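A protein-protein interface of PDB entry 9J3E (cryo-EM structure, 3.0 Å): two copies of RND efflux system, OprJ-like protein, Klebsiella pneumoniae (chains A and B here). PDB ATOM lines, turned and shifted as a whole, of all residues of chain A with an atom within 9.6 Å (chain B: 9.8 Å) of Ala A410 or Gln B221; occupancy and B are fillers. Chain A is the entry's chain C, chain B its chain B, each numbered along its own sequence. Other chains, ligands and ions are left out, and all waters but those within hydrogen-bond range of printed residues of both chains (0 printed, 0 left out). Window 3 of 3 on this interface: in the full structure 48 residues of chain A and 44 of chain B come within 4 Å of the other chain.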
ATOM      1  N   GLN A 402      10.773 -31.104 -23.112  1.00  0.00           N
ATOM      2  CA  GLN A 402       9.670 -31.806 -22.472  1.00  0.00           C
ATOM      3  C   GLN A 402       8.672 -30.822 -21.882  1.00  0.00           C
ATOM      4  O   GLN A 402       7.458 -31.022 -21.984  1.00  0.00           O
ATOM      5  CB  GLN A 402      10.213 -32.735 -21.391  1.00  0.00           C
ATOM      6  CG  GLN A 402       9.211 -33.717 -20.849  1.00  0.00           C
ATOM      7  CD  GLN A 402       8.305 -34.262 -21.921  1.00  0.00           C
ATOM      8  OE1 GLN A 402       7.191 -33.781 -22.114  1.00  0.00           O
ATOM      9  NE2 GLN A 402       8.785 -35.267 -22.640  1.00  0.00           N
ATOM     10  N   ALA A 403       9.167 -29.752 -21.258  1.00  0.00           N
ATOM     11  CA  ALA A 403       8.263 -28.717 -20.772  1.00  0.00           C
ATOM     12  C   ALA A 403       7.484 -28.092 -21.920  1.00  0.00           C
ATOM     13  O   ALA A 403       6.282 -27.833 -21.801  1.00  0.00           O
ATOM     14  CB  ALA A 403       9.042 -27.650 -20.008  1.00  0.00           C
ATOM     15  N   LEU A 404       8.155 -27.851 -23.045  1.00  0.00           N
ATOM     16  CA  LEU A 404       7.482 -27.297 -24.216  1.00  0.00           C
ATOM     17  C   LEU A 404       6.405 -28.240 -24.740  1.00  0.00           C
ATOM     18  O   LEU A 404       5.307 -27.802 -25.108  1.00  0.00           O
ATOM     19  CB  LEU A 404       8.508 -27.002 -25.303  1.00  0.00           C
ATOM     20  CG  LEU A 404       7.983 -26.647 -26.690  1.00  0.00           C
ATOM     21  CD1 LEU A 404       7.127 -25.409 -26.635  1.00  0.00           C
ATOM     22  CD2 LEU A 404       9.136 -26.449 -27.650  1.00  0.00           C
ATOM     23  N   ALA A 405       6.707 -29.535 -24.801  1.00  0.00           N
ATOM     24  CA  ALA A 405       5.716 -30.498 -25.263  1.00  0.00           C
ATOM     25  C   ALA A 405       4.529 -30.554 -24.317  1.00  0.00           C
ATOM     26  O   ALA A 405       3.378 -30.652 -24.755  1.00  0.00           O
ATOM     27  CB  ALA A 405       6.350 -31.876 -25.412  1.00  0.00           C
ATOM     28  N   GLY A 406       4.786 -30.490 -23.012  1.00  0.00           N
ATOM     29  CA  GLY A 406       3.691 -30.422 -22.063  1.00  0.00           C
ATOM     30  C   GLY A 406       2.845 -29.181 -22.255  1.00  0.00           C
ATOM     31  O   GLY A 406       1.622 -29.221 -22.115  1.00  0.00           O
ATOM     32  N   SER A 407       3.487 -28.058 -22.574  1.00  0.00           N
ATOM     33  CA  SER A 407       2.741 -26.834 -22.841  1.00  0.00           C
ATOM     34  C   SER A 407       1.847 -26.983 -24.062  1.00  0.00           C
ATOM     35  O   SER A 407       0.680 -26.570 -24.046  1.00  0.00           O
ATOM     36  CB  SER A 407       3.703 -25.668 -23.028  1.00  0.00           C
ATOM     37  OG  SER A 407       2.993 -24.492 -23.358  1.00  0.00           O
ATOM     38  N   SER A 408       2.372 -27.565 -25.136  1.00  0.00           N
ATOM     39  CA  SER A 408       1.538 -27.763 -26.318  1.00  0.00           C
ATOM     40  C   SER A 408       0.414 -28.752 -26.033  1.00  0.00           C
ATOM     41  O   SER A 408      -0.679 -28.643 -26.597  1.00  0.00           O
ATOM     42  CB  SER A 408       2.387 -28.221 -27.499  1.00  0.00           C
ATOM     43  OG  SER A 408       3.083 -29.412 -27.198  1.00  0.00           O
ATOM     44  N   GLU A 409       0.646 -29.705 -25.132  1.00  0.00           N
ATOM     45  CA  GLU A 409      -0.416 -30.640 -24.779  1.00  0.00           C
ATOM     46  C   GLU A 409      -1.491 -29.965 -23.933  1.00  0.00           C
ATOM     47  O   GLU A 409      -2.677 -30.298 -24.032  1.00  0.00           O
ATOM     48  CB  GLU A 409       0.179 -31.836 -24.044  1.00  0.00           C
ATOM     49  CG  GLU A 409       0.178 -33.114 -24.856  1.00  0.00           C
ATOM     50  CD  GLU A 409      -1.217 -33.601 -25.178  1.00  0.00           C
ATOM     51  OE1 GLU A 409      -2.165 -33.221 -24.461  1.00  0.00           O
ATOM     52  OE2 GLU A 409      -1.366 -34.367 -26.153  1.00  0.00           O
ATOM     53  N   ALA A 410      -1.093 -29.021 -23.083  1.00  0.00           N
ATOM     54  CA  ALA A 410      -2.081 -28.211 -22.379  1.00  0.00           C
ATOM     55  C   ALA A 410      -2.892 -27.385 -23.363  1.00  0.00           C
ATOM     56  O   ALA A 410      -4.112 -27.225 -23.209  1.00  0.00           O
ATOM     57  CB  ALA A 410      -1.389 -27.314 -21.356  1.00  0.00           C
ATOM     58  N   ALA A 411      -2.226 -26.855 -24.389  1.00  0.00           N
ATOM     59  CA  ALA A 411      -2.942 -26.185 -25.465  1.00  0.00           C
ATOM     60  C   ALA A 411      -3.926 -27.132 -26.136  1.00  0.00           C
ATOM     61  O   ALA A 411      -5.018 -26.723 -26.530  1.00  0.00           O
ATOM     62  CB  ALA A 411      -1.952 -25.628 -26.483  1.00  0.00           C
ATOM     63  N   MET A 412      -3.545 -28.401 -26.294  1.00  0.00           N
ATOM     64  CA  MET A 412      -4.471 -29.420 -26.787  1.00  0.00           C
ATOM     65  C   MET A 412      -5.704 -29.541 -25.914  1.00  0.00           C
ATOM     66  O   MET A 412      -6.832 -29.543 -26.410  1.00  0.00           O
ATOM     67  CB  MET A 412      -3.773 -30.779 -26.869  1.00  0.00           C
ATOM     68  CG  MET A 412      -4.306 -31.734 -27.930  1.00  0.00           C
ATOM     69  SD  MET A 412      -5.040 -30.896 -29.327  1.00  0.00           S
ATOM     70  CE  MET A 412      -3.604 -29.988 -29.841  1.00  0.00           C
ATOM     71  N   ALA A 413      -5.501 -29.688 -24.609  1.00  0.00           N
ATOM     72  CA  ALA A 413      -6.642 -29.817 -23.715  1.00  0.00           C
ATOM     73  C   ALA A 413      -7.576 -28.629 -23.869  1.00  0.00           C
ATOM     74  O   ALA A 413      -8.791 -28.797 -24.023  1.00  0.00           O
ATOM     75  CB  ALA A 413      -6.171 -29.943 -22.269  1.00  0.00           C
ATOM     76  N   LEU A 414      -7.015 -27.421 -23.893  1.00  0.00           N
ATOM     77  CA  LEU A 414      -7.851 -26.229 -23.974  1.00  0.00           C
ATOM     78  C   LEU A 414      -8.542 -26.107 -25.326  1.00  0.00           C
ATOM     79  O   LEU A 414      -9.739 -25.806 -25.391  1.00  0.00           O
ATOM     80  CB  LEU A 414      -7.014 -24.994 -23.676  1.00  0.00           C
ATOM     81  CG  LEU A 414      -6.559 -24.988 -22.223  1.00  0.00           C
ATOM     82  CD1 LEU A 414      -5.497 -23.950 -22.002  1.00  0.00           C
ATOM     83  CD2 LEU A 414      -7.748 -24.729 -21.329  1.00  0.00           C
ATOM     84  N   ALA A 415      -7.809 -26.321 -26.417  1.00  0.00           N
ATOM     85  CA  ALA A 415      -8.398 -26.188 -27.743  1.00  0.00           C
ATOM     86  C   ALA A 415      -9.474 -27.236 -27.973  1.00  0.00           C
ATOM     87  O   ALA A 415     -10.516 -26.941 -28.564  1.00  0.00           O
ATOM     88  CB  ALA A 415      -7.314 -26.287 -28.811  1.00  0.00           C
ATOM     89  N   LYS A 416      -9.242 -28.465 -27.518  1.00  0.00           N
ATOM     90  CA  LYS A 416     -10.266 -29.492 -27.630  1.00  0.00           C
ATOM     91  C   LYS A 416     -11.481 -29.145 -26.790  1.00  0.00           C
ATOM     92  O   LYS A 416     -12.617 -29.341 -27.227  1.00  0.00           O
ATOM     93  CB  LYS A 416      -9.698 -30.846 -27.217  1.00  0.00           C
ATOM     94  CG  LYS A 416     -10.753 -31.865 -26.850  1.00  0.00           C
ATOM     95  CD  LYS A 416     -10.437 -33.220 -27.444  1.00  0.00           C
ATOM     96  CE  LYS A 416     -11.078 -34.331 -26.638  1.00  0.00           C
ATOM     97  NZ  LYS A 416     -10.293 -34.624 -25.411  1.00  0.00           N
ATOM     98  N   ALA A 417     -11.268 -28.620 -25.583  1.00  0.00           N
ATOM     99  CA  ALA A 417     -12.405 -28.224 -24.762  1.00  0.00           C
ATOM    100  C   ALA A 417     -13.221 -27.147 -25.455  1.00  0.00           C
ATOM    101  O   ALA A 417     -14.455 -27.176 -25.426  1.00  0.00           O
ATOM    102  CB  ALA A 417     -11.925 -27.737 -23.399  1.00  0.00           C
ATOM    103  N   ARG A 418     -12.546 -26.189 -26.085  1.00  0.00           N
ATOM    104  CA  ARG A 418     -13.256 -25.148 -26.814  1.00  0.00           C
ATOM    105  C   ARG A 418     -14.011 -25.724 -28.003  1.00  0.00           C
ATOM    106  O   ARG A 418     -15.172 -25.376 -28.236  1.00  0.00           O
ATOM    107  CB  ARG A 418     -12.276 -24.081 -27.276  1.00  0.00           C
ATOM    108  CG  ARG A 418     -11.751 -23.222 -26.161  1.00  0.00           C
ATOM    109  CD  ARG A 418     -10.758 -22.233 -26.699  1.00  0.00           C
ATOM    110  NE  ARG A 418     -11.403 -21.293 -27.601  1.00  0.00           N
ATOM    111  CZ  ARG A 418     -11.429 -19.982 -27.416  1.00  0.00           C
ATOM    112  NH1 ARG A 418     -10.843 -19.421 -26.375  1.00  0.00           N
ATOM    113  NH2 ARG A 418     -12.063 -19.217 -28.299  1.00  0.00           N
ATOM    114  N   TYR A 429      -8.780 -26.565 -33.802  1.00  0.00           N
ATOM    115  CA  TYR A 429      -8.365 -27.786 -33.128  1.00  0.00           C
ATOM    116  C   TYR A 429      -7.285 -28.509 -33.919  1.00  0.00           C
ATOM    117  O   TYR A 429      -6.290 -28.972 -33.350  1.00  0.00           O
ATOM    118  CB  TYR A 429      -9.571 -28.694 -32.925  1.00  0.00           C
ATOM    119  CG  TYR A 429      -9.223 -30.056 -32.401  1.00  0.00           C
ATOM    120  CD1 TYR A 429      -8.490 -30.203 -31.239  1.00  0.00           C
ATOM    121  CD2 TYR A 429      -9.613 -31.193 -33.077  1.00  0.00           C
ATOM    122  CE1 TYR A 429      -8.171 -31.449 -30.757  1.00  0.00           C
ATOM    123  CE2 TYR A 429      -9.297 -32.442 -32.607  1.00  0.00           C
ATOM    124  CZ  TYR A 429      -8.576 -32.565 -31.447  1.00  0.00           C
ATOM    125  OH  TYR A 429      -8.256 -33.815 -30.973  1.00  0.00           O
ATOM    126  N   ALA A 432      -3.999 -26.707 -33.623  1.00  0.00           N
ATOM    127  CA  ALA A 432      -3.371 -27.017 -32.349  1.00  0.00           C
ATOM    128  C   ALA A 432      -2.736 -28.400 -32.381  1.00  0.00           C
ATOM    129  O   ALA A 432      -1.645 -28.600 -31.834  1.00  0.00           O
ATOM    130  CB  ALA A 432      -4.396 -26.910 -31.223  1.00  0.00           C
ATOM    131  N   SER A 435       0.506 -28.231 -34.177  1.00  0.00           N
ATOM    132  CA  SER A 435       1.497 -27.564 -33.343  1.00  0.00           C
ATOM    133  C   SER A 435       2.058 -28.512 -32.294  1.00  0.00           C
ATOM    134  O   SER A 435       3.282 -28.629 -32.134  1.00  0.00           O
ATOM    135  CB  SER A 435       0.875 -26.339 -32.681  1.00  0.00           C
ATOM    136  OG  SER A 435       1.818 -25.667 -31.871  1.00  0.00           O
ATOM    137  N   THR A 436       1.178 -29.206 -31.571  1.00  0.00           N
ATOM    138  CA  THR A 436       1.659 -30.080 -30.508  1.00  0.00           C
ATOM    139  C   THR A 436       2.470 -31.230 -31.066  1.00  0.00           C
ATOM    140  O   THR A 436       3.410 -31.700 -30.419  1.00  0.00           O
ATOM    141  CB  THR A 436       0.510 -30.620 -29.657  1.00  0.00           C
ATOM    142  OG1 THR A 436       1.056 -31.358 -28.561  1.00  0.00           O
ATOM    143  CG2 THR A 436      -0.360 -31.555 -30.443  1.00  0.00           C
ATOM    144  N   ASN A 439       5.909 -30.028 -31.854  1.00  0.00           N
ATOM    145  CA  ASN A 439       6.678 -29.930 -30.618  1.00  0.00           C
ATOM    146  C   ASN A 439       7.124 -31.306 -30.147  1.00  0.00           C
ATOM    147  O   ASN A 439       8.262 -31.483 -29.697  1.00  0.00           O
ATOM    148  CB  ASN A 439       5.860 -29.229 -29.539  1.00  0.00           C
ATOM    149  CG  ASN A 439       5.638 -27.768 -29.841  1.00  0.00           C
ATOM    150  OD1 ASN A 439       4.652 -27.177 -29.412  1.00  0.00           O
ATOM    151  ND2 ASN A 439       6.561 -27.175 -30.582  1.00  0.00           N
ATOM    152  N   SER B 202       8.334 -11.544 -20.186  1.00  0.00           N
ATOM    153  CA  SER B 202       7.040 -11.623 -20.857  1.00  0.00           C
ATOM    154  C   SER B 202       6.182 -12.734 -20.270  1.00  0.00           C
ATOM    155  O   SER B 202       4.964 -12.588 -20.151  1.00  0.00           O
ATOM    156  CB  SER B 202       7.225 -11.828 -22.356  1.00  0.00           C
ATOM    157  OG  SER B 202       8.232 -10.977 -22.863  1.00  0.00           O
ATOM    158  N   LEU B 203       6.798 -13.859 -19.911  1.00  0.00           N
ATOM    159  CA  LEU B 203       6.047 -14.955 -19.317  1.00  0.00           C
ATOM    160  C   LEU B 203       5.440 -14.547 -17.988  1.00  0.00           C
ATOM    161  O   LEU B 203       4.273 -14.838 -17.721  1.00  0.00           O
ATOM    162  CB  LEU B 203       6.947 -16.171 -19.130  1.00  0.00           C
ATOM    163  CG  LEU B 203       6.327 -17.316 -18.338  1.00  0.00           C
ATOM    164  CD1 LEU B 203       5.018 -17.720 -18.960  1.00  0.00           C
ATOM    165  CD2 LEU B 203       7.272 -18.494 -18.281  1.00  0.00           C
ATOM    166  N   VAL B 206       2.522 -12.086 -18.715  1.00  0.00           N
ATOM    167  CA  VAL B 206       1.336 -12.785 -19.194  1.00  0.00           C
ATOM    168  C   VAL B 206       0.724 -13.625 -18.084  1.00  0.00           C
ATOM    169  O   VAL B 206      -0.498 -13.785 -18.011  1.00  0.00           O
ATOM    170  CB  VAL B 206       1.685 -13.634 -20.426  1.00  0.00           C
ATOM    171  CG1 VAL B 206       0.542 -14.555 -20.775  1.00  0.00           C
ATOM    172  CG2 VAL B 206       2.007 -12.735 -21.599  1.00  0.00           C
ATOM    173  N   SER B 207       1.556 -14.188 -17.212  1.00  0.00           N
ATOM    174  CA  SER B 207       1.035 -14.914 -16.065  1.00  0.00           C
ATOM    175  C   SER B 207       0.214 -13.995 -15.177  1.00  0.00           C
ATOM    176  O   SER B 207      -0.852 -14.378 -14.685  1.00  0.00           O
ATOM    177  CB  SER B 207       2.185 -15.534 -15.277  1.00  0.00           C
ATOM    178  OG  SER B 207       1.704 -16.307 -14.197  1.00  0.00           O
ATOM    179  N   ARG B 210      -3.135 -13.304 -17.002  1.00  0.00           N
ATOM    180  CA  ARG B 210      -4.063 -14.414 -16.825  1.00  0.00           C
ATOM    181  C   ARG B 210      -4.603 -14.450 -15.407  1.00  0.00           C
ATOM    182  O   ARG B 210      -5.792 -14.706 -15.193  1.00  0.00           O
ATOM    183  CB  ARG B 210      -3.395 -15.744 -17.150  1.00  0.00           C
ATOM    184  CG  ARG B 210      -4.328 -16.908 -16.912  1.00  0.00           C
ATOM    185  CD  ARG B 210      -3.607 -18.144 -16.441  1.00  0.00           C
ATOM    186  NE  ARG B 210      -4.557 -19.146 -15.974  1.00  0.00           N
ATOM    187  CZ  ARG B 210      -4.409 -20.455 -16.128  1.00  0.00           C
ATOM    188  NH1 ARG B 210      -3.352 -20.964 -16.737  1.00  0.00           N
ATOM    189  NH2 ARG B 210      -5.348 -21.271 -15.660  1.00  0.00           N
ATOM    190  N   ALA B 215      -6.428 -12.344 -19.760  1.00  0.00           N
ATOM    191  CA  ALA B 215      -5.835 -13.192 -20.782  1.00  0.00           C
ATOM    192  C   ALA B 215      -6.284 -14.631 -20.592  1.00  0.00           C
ATOM    193  O   ALA B 215      -6.471 -15.099 -19.469  1.00  0.00           O
ATOM    194  CB  ALA B 215      -4.307 -13.123 -20.750  1.00  0.00           C
ATOM    195  N   THR B 216      -6.448 -15.333 -21.706  1.00  0.00           N
ATOM    196  CA  THR B 216      -6.829 -16.732 -21.661  1.00  0.00           C
ATOM    197  C   THR B 216      -5.643 -17.590 -21.247  1.00  0.00           C
ATOM    198  O   THR B 216      -4.491 -17.152 -21.263  1.00  0.00           O
ATOM    199  CB  THR B 216      -7.337 -17.206 -23.016  1.00  0.00           C
ATOM    200  OG1 THR B 216      -6.222 -17.572 -23.834  1.00  0.00           O
ATOM    201  CG2 THR B 216      -8.109 -16.101 -23.707  1.00  0.00           C
ATOM    202  N   ALA B 217      -5.936 -18.833 -20.873  1.00  0.00           N
ATOM    203  CA  ALA B 217      -4.863 -19.770 -20.579  1.00  0.00           C
ATOM    204  C   ALA B 217      -4.060 -20.118 -21.819  1.00  0.00           C
ATOM    205  O   ALA B 217      -2.915 -20.559 -21.695  1.00  0.00           O
ATOM    206  CB  ALA B 217      -5.423 -21.043 -19.951  1.00  0.00           C
ATOM    207  N   LEU B 218      -4.630 -19.928 -23.008  1.00  0.00           N
ATOM    208  CA  LEU B 218      -3.885 -20.176 -24.235  1.00  0.00           C
ATOM    209  C   LEU B 218      -2.687 -19.249 -24.349  1.00  0.00           C
ATOM    210  O   LEU B 218      -1.596 -19.675 -24.746  1.00  0.00           O
ATOM    211  CB  LEU B 218      -4.801 -19.997 -25.440  1.00  0.00           C
ATOM    212  CG  LEU B 218      -5.934 -21.000 -25.579  1.00  0.00           C
ATOM    213  CD1 LEU B 218      -6.471 -20.973 -26.988  1.00  0.00           C
ATOM    214  CD2 LEU B 218      -5.407 -22.364 -25.253  1.00  0.00           C
ATOM    215  N   ASP B 219      -2.874 -17.971 -24.023  1.00  0.00           N
ATOM    216  CA  ASP B 219      -1.760 -17.036 -24.077  1.00  0.00           C
ATOM    217  C   ASP B 219      -0.692 -17.402 -23.062  1.00  0.00           C
ATOM    218  O   ASP B 219       0.505 -17.328 -23.358  1.00  0.00           O
ATOM    219  CB  ASP B 219      -2.259 -15.612 -23.851  1.00  0.00           C
ATOM    220  CG  ASP B 219      -3.319 -15.211 -24.849  1.00  0.00           C
ATOM    221  OD1 ASP B 219      -3.150 -15.524 -26.044  1.00  0.00           O
ATOM    222  OD2 ASP B 219      -4.316 -14.582 -24.445  1.00  0.00           O
ATOM    223  N   TYR B 220      -1.102 -17.809 -21.865  1.00  0.00           N
ATOM    224  CA  TYR B 220      -0.123 -18.227 -20.877  1.00  0.00           C
ATOM    225  C   TYR B 220       0.648 -19.440 -21.374  1.00  0.00           C
ATOM    226  O   TYR B 220       1.868 -19.525 -21.208  1.00  0.00           O
ATOM    227  CB  TYR B 220      -0.813 -18.539 -19.555  1.00  0.00           C
ATOM    228  CG  TYR B 220       0.112 -19.135 -18.533  1.00  0.00           C
ATOM    229  CD1 TYR B 220      -0.281 -20.199 -17.743  1.00  0.00           C
ATOM    230  CD2 TYR B 220       1.366 -18.592 -18.320  1.00  0.00           C
ATOM    231  CE1 TYR B 220       0.567 -20.731 -16.802  1.00  0.00           C
ATOM    232  CE2 TYR B 220       2.213 -19.109 -17.382  1.00  0.00           C
ATOM    233  CZ  TYR B 220       1.813 -20.178 -16.626  1.00  0.00           C
ATOM    234  OH  TYR B 220       2.672 -20.693 -15.686  1.00  0.00           O
ATOM    235  N   GLN B 221      -0.051 -20.385 -22.006  1.00  0.00           N
ATOM    236  CA  GLN B 221       0.610 -21.583 -22.509  1.00  0.00           C
ATOM    237  C   GLN B 221       1.601 -21.252 -23.612  1.00  0.00           C
ATOM    238  O   GLN B 221       2.705 -21.803 -23.646  1.00  0.00           O
ATOM    239  CB  GLN B 221      -0.424 -22.580 -23.018  1.00  0.00           C
ATOM    240  CG  GLN B 221      -1.219 -23.243 -21.929  1.00  0.00           C
ATOM    241  CD  GLN B 221      -0.352 -24.018 -20.976  1.00  0.00           C
ATOM    242  OE1 GLN B 221       0.725 -24.483 -21.337  1.00  0.00           O
ATOM    243  NE2 GLN B 221      -0.818 -24.167 -19.747  1.00  0.00           N
ATOM    244  N   GLU B 222       1.226 -20.369 -24.535  1.00  0.00           N
ATOM    245  CA  GLU B 222       2.150 -20.046 -25.615  1.00  0.00           C
ATOM    246  C   GLU B 222       3.343 -19.254 -25.093  1.00  0.00           C
ATOM    247  O   GLU B 222       4.466 -19.421 -25.583  1.00  0.00           O
ATOM    248  CB  GLU B 222       1.430 -19.298 -26.736  1.00  0.00           C
ATOM    249  CG  GLU B 222       0.891 -17.947 -26.360  1.00  0.00           C
ATOM    250  CD  GLU B 222       1.847 -16.830 -26.705  1.00  0.00           C
ATOM    251  OE1 GLU B 222       2.960 -17.131 -27.179  1.00  0.00           O
ATOM    252  OE2 GLU B 222       1.488 -15.652 -26.496  1.00  0.00           O
ATOM    253  N   ALA B 223       3.133 -18.406 -24.084  1.00  0.00           N
ATOM    254  CA  ALA B 223       4.266 -17.739 -23.450  1.00  0.00           C
ATOM    255  C   ALA B 223       5.187 -18.750 -22.784  1.00  0.00           C
ATOM    256  O   ALA B 223       6.416 -18.628 -22.858  1.00  0.00           O
ATOM    257  CB  ALA B 223       3.776 -16.713 -22.435  1.00  0.00           C
ATOM    258  N   VAL B 224       4.612 -19.754 -22.124  1.00  0.00           N
ATOM    259  CA  VAL B 224       5.423 -20.804 -21.521  1.00  0.00           C
ATOM    260  C   VAL B 224       6.229 -21.524 -22.588  1.00  0.00           C
ATOM    261  O   VAL B 224       7.421 -21.792 -22.414  1.00  0.00           O
ATOM    262  CB  VAL B 224       4.536 -21.783 -20.732  1.00  0.00           C
ATOM    263  CG1 VAL B 224       5.271 -23.078 -20.487  1.00  0.00           C
ATOM    264  CG2 VAL B 224       4.129 -21.174 -19.423  1.00  0.00           C
ATOM    265  N   GLY B 225       5.588 -21.850 -23.707  1.00  0.00           N
ATOM    266  CA  GLY B 225       6.297 -22.520 -24.780  1.00  0.00           C
ATOM    267  C   GLY B 225       7.435 -21.684 -25.325  1.00  0.00           C
ATOM    268  O   GLY B 225       8.514 -22.200 -25.619  1.00  0.00           O
ATOM    269  N   LEU B 226       7.211 -20.379 -25.464  1.00  0.00           N
ATOM    270  CA  LEU B 226       8.267 -19.494 -25.940  1.00  0.00           C
ATOM    271  C   LEU B 226       9.432 -19.446 -24.960  1.00  0.00           C
ATOM    272  O   LEU B 226      10.601 -19.462 -25.367  1.00  0.00           O
ATOM    273  CB  LEU B 226       7.691 -18.104 -26.181  1.00  0.00           C
ATOM    274  CG  LEU B 226       6.720 -18.026 -27.360  1.00  0.00           C
ATOM    275  CD1 LEU B 226       6.691 -16.637 -27.956  1.00  0.00           C
ATOM    276  CD2 LEU B 226       7.107 -19.035 -28.424  1.00  0.00           C
ATOM    277  N   ALA B 227       9.135 -19.390 -23.661  1.00  0.00           N
ATOM    278  CA  ALA B 227      10.201 -19.402 -22.666  1.00  0.00           C
ATOM    279  C   ALA B 227      10.984 -20.708 -22.716  1.00  0.00           C
ATOM    280  O   ALA B 227      12.216 -20.708 -22.616  1.00  0.00           O
ATOM    281  CB  ALA B 227       9.622 -19.178 -21.274  1.00  0.00           C
ATOM    282  N   GLU B 228      10.285 -21.833 -22.874  1.00  0.00           N
ATOM    283  CA  GLU B 228      10.974 -23.114 -22.983  1.00  0.00           C
ATOM    284  C   GLU B 228      11.849 -23.156 -24.226  1.00  0.00           C
ATOM    285  O   GLU B 228      12.958 -23.698 -24.198  1.00  0.00           O
ATOM    286  CB  GLU B 228       9.969 -24.263 -23.012  1.00  0.00           C
ATOM    287  CG  GLU B 228       9.018 -24.310 -21.838  1.00  0.00           C
ATOM    288  CD  GLU B 228       9.719 -24.211 -20.506  1.00  0.00           C
ATOM    289  OE1 GLU B 228      10.781 -24.843 -20.336  1.00  0.00           O
ATOM    290  OE2 GLU B 228       9.203 -23.500 -19.621  1.00  0.00           O
ATOM    291  N   GLN B 229      11.356 -22.602 -25.331  1.00  0.00           N
ATOM    292  CA  GLN B 229      12.141 -22.568 -26.556  1.00  0.00           C
ATOM    293  C   GLN B 229      13.408 -21.749 -26.365  1.00  0.00           C
ATOM    294  O   GLN B 229      14.494 -22.151 -26.804  1.00  0.00           O
ATOM    295  CB  GLN B 229      11.287 -22.005 -27.689  1.00  0.00           C
ATOM    296  CG  GLN B 229      11.767 -22.347 -29.080  1.00  0.00           C
ATOM    297  CD  GLN B 229      12.896 -21.460 -29.531  1.00  0.00           C
ATOM    298  OE1 GLN B 229      12.893 -20.257 -29.274  1.00  0.00           O
ATOM    299  NE2 GLN B 229      13.876 -22.045 -30.209  1.00  0.00           N
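No position is printed for both chains. Of the 9 pairs that touch across the chains among the printed residues, none has its exchanged pair printed and touching as well.
The backbone carbonyl oxygen of Gln B221 sits at hydrogen-bond distance from the side-chain hydroxyl of Ser A407, 2.7 Å away.
Hydrophobic or aromatic side chains of chain A within 4 Å of the printed part of chain B: Ala A403, Leu A404, Ala A410 and Leu A414. Of the 20 printed residues of chain B, 6 touch a printed residue of chain A. Printed residues of chain B that touch a printed residue of chain A: Ala B217, Leu B218, Gln B221, Val B224, Gly B225 and Glu B228. Among the printed residues, no Asp or Glu carboxylate lies within 4 Å of a Lys or Arg side-chain nitrogen of the other chain.
Among the printed residues, pairs that only touch across the chains: Ala A403 with Glu B228, Leu A414 with Leu B218, Ala A410 with Gln B221, Leu A404 with Gly B225, Leu A414 with Ala B217, Ser A407 with Gly B225, Leu A404 with Glu B228 and Ser A407 with Val B224.
Ala A410 touches just one residue of chain B: Gln B221 (3.5 Å). Gln B221 touches just these residues of chain A: Ser A407 and Ala A410. Of chain B, only Gln B221, Val B224 and Gly B225 come within 4 Å of Ser A407. No residue of chain B comes within 4 Å of Ala A411. No residue of chain B comes within 4 Å of Ala A413. Printed residues of chain B within 4 Å of Ala A403: Glu B228. Printed residues of chain A within 4 Å of Glu B228: Ala A403 (3.3 Å) and Leu A404 (3.8 Å). Of the printed residues of chain B, Leu A404 touches Gly B225 and Glu B228. Arg B210 touches none of the printed residues of chain A. The nearest residue of chain B that does not touch Ala A410 is Leu B218 (5.4 Å). The nearest residue of chain A that does not touch Gln B221 is Leu A414 (4.3 Å).
The side-chain hydroxyl (OG) of Ser A408 lies within hydrogen-bond range of the backbone carbonyl oxygen (O) of Leu A404, 3.5 Å away. The side-chain hydroxyl of Thr B216 lies within hydrogen-bond range of the backbone NH of Leu B218, 3.0 Å away.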
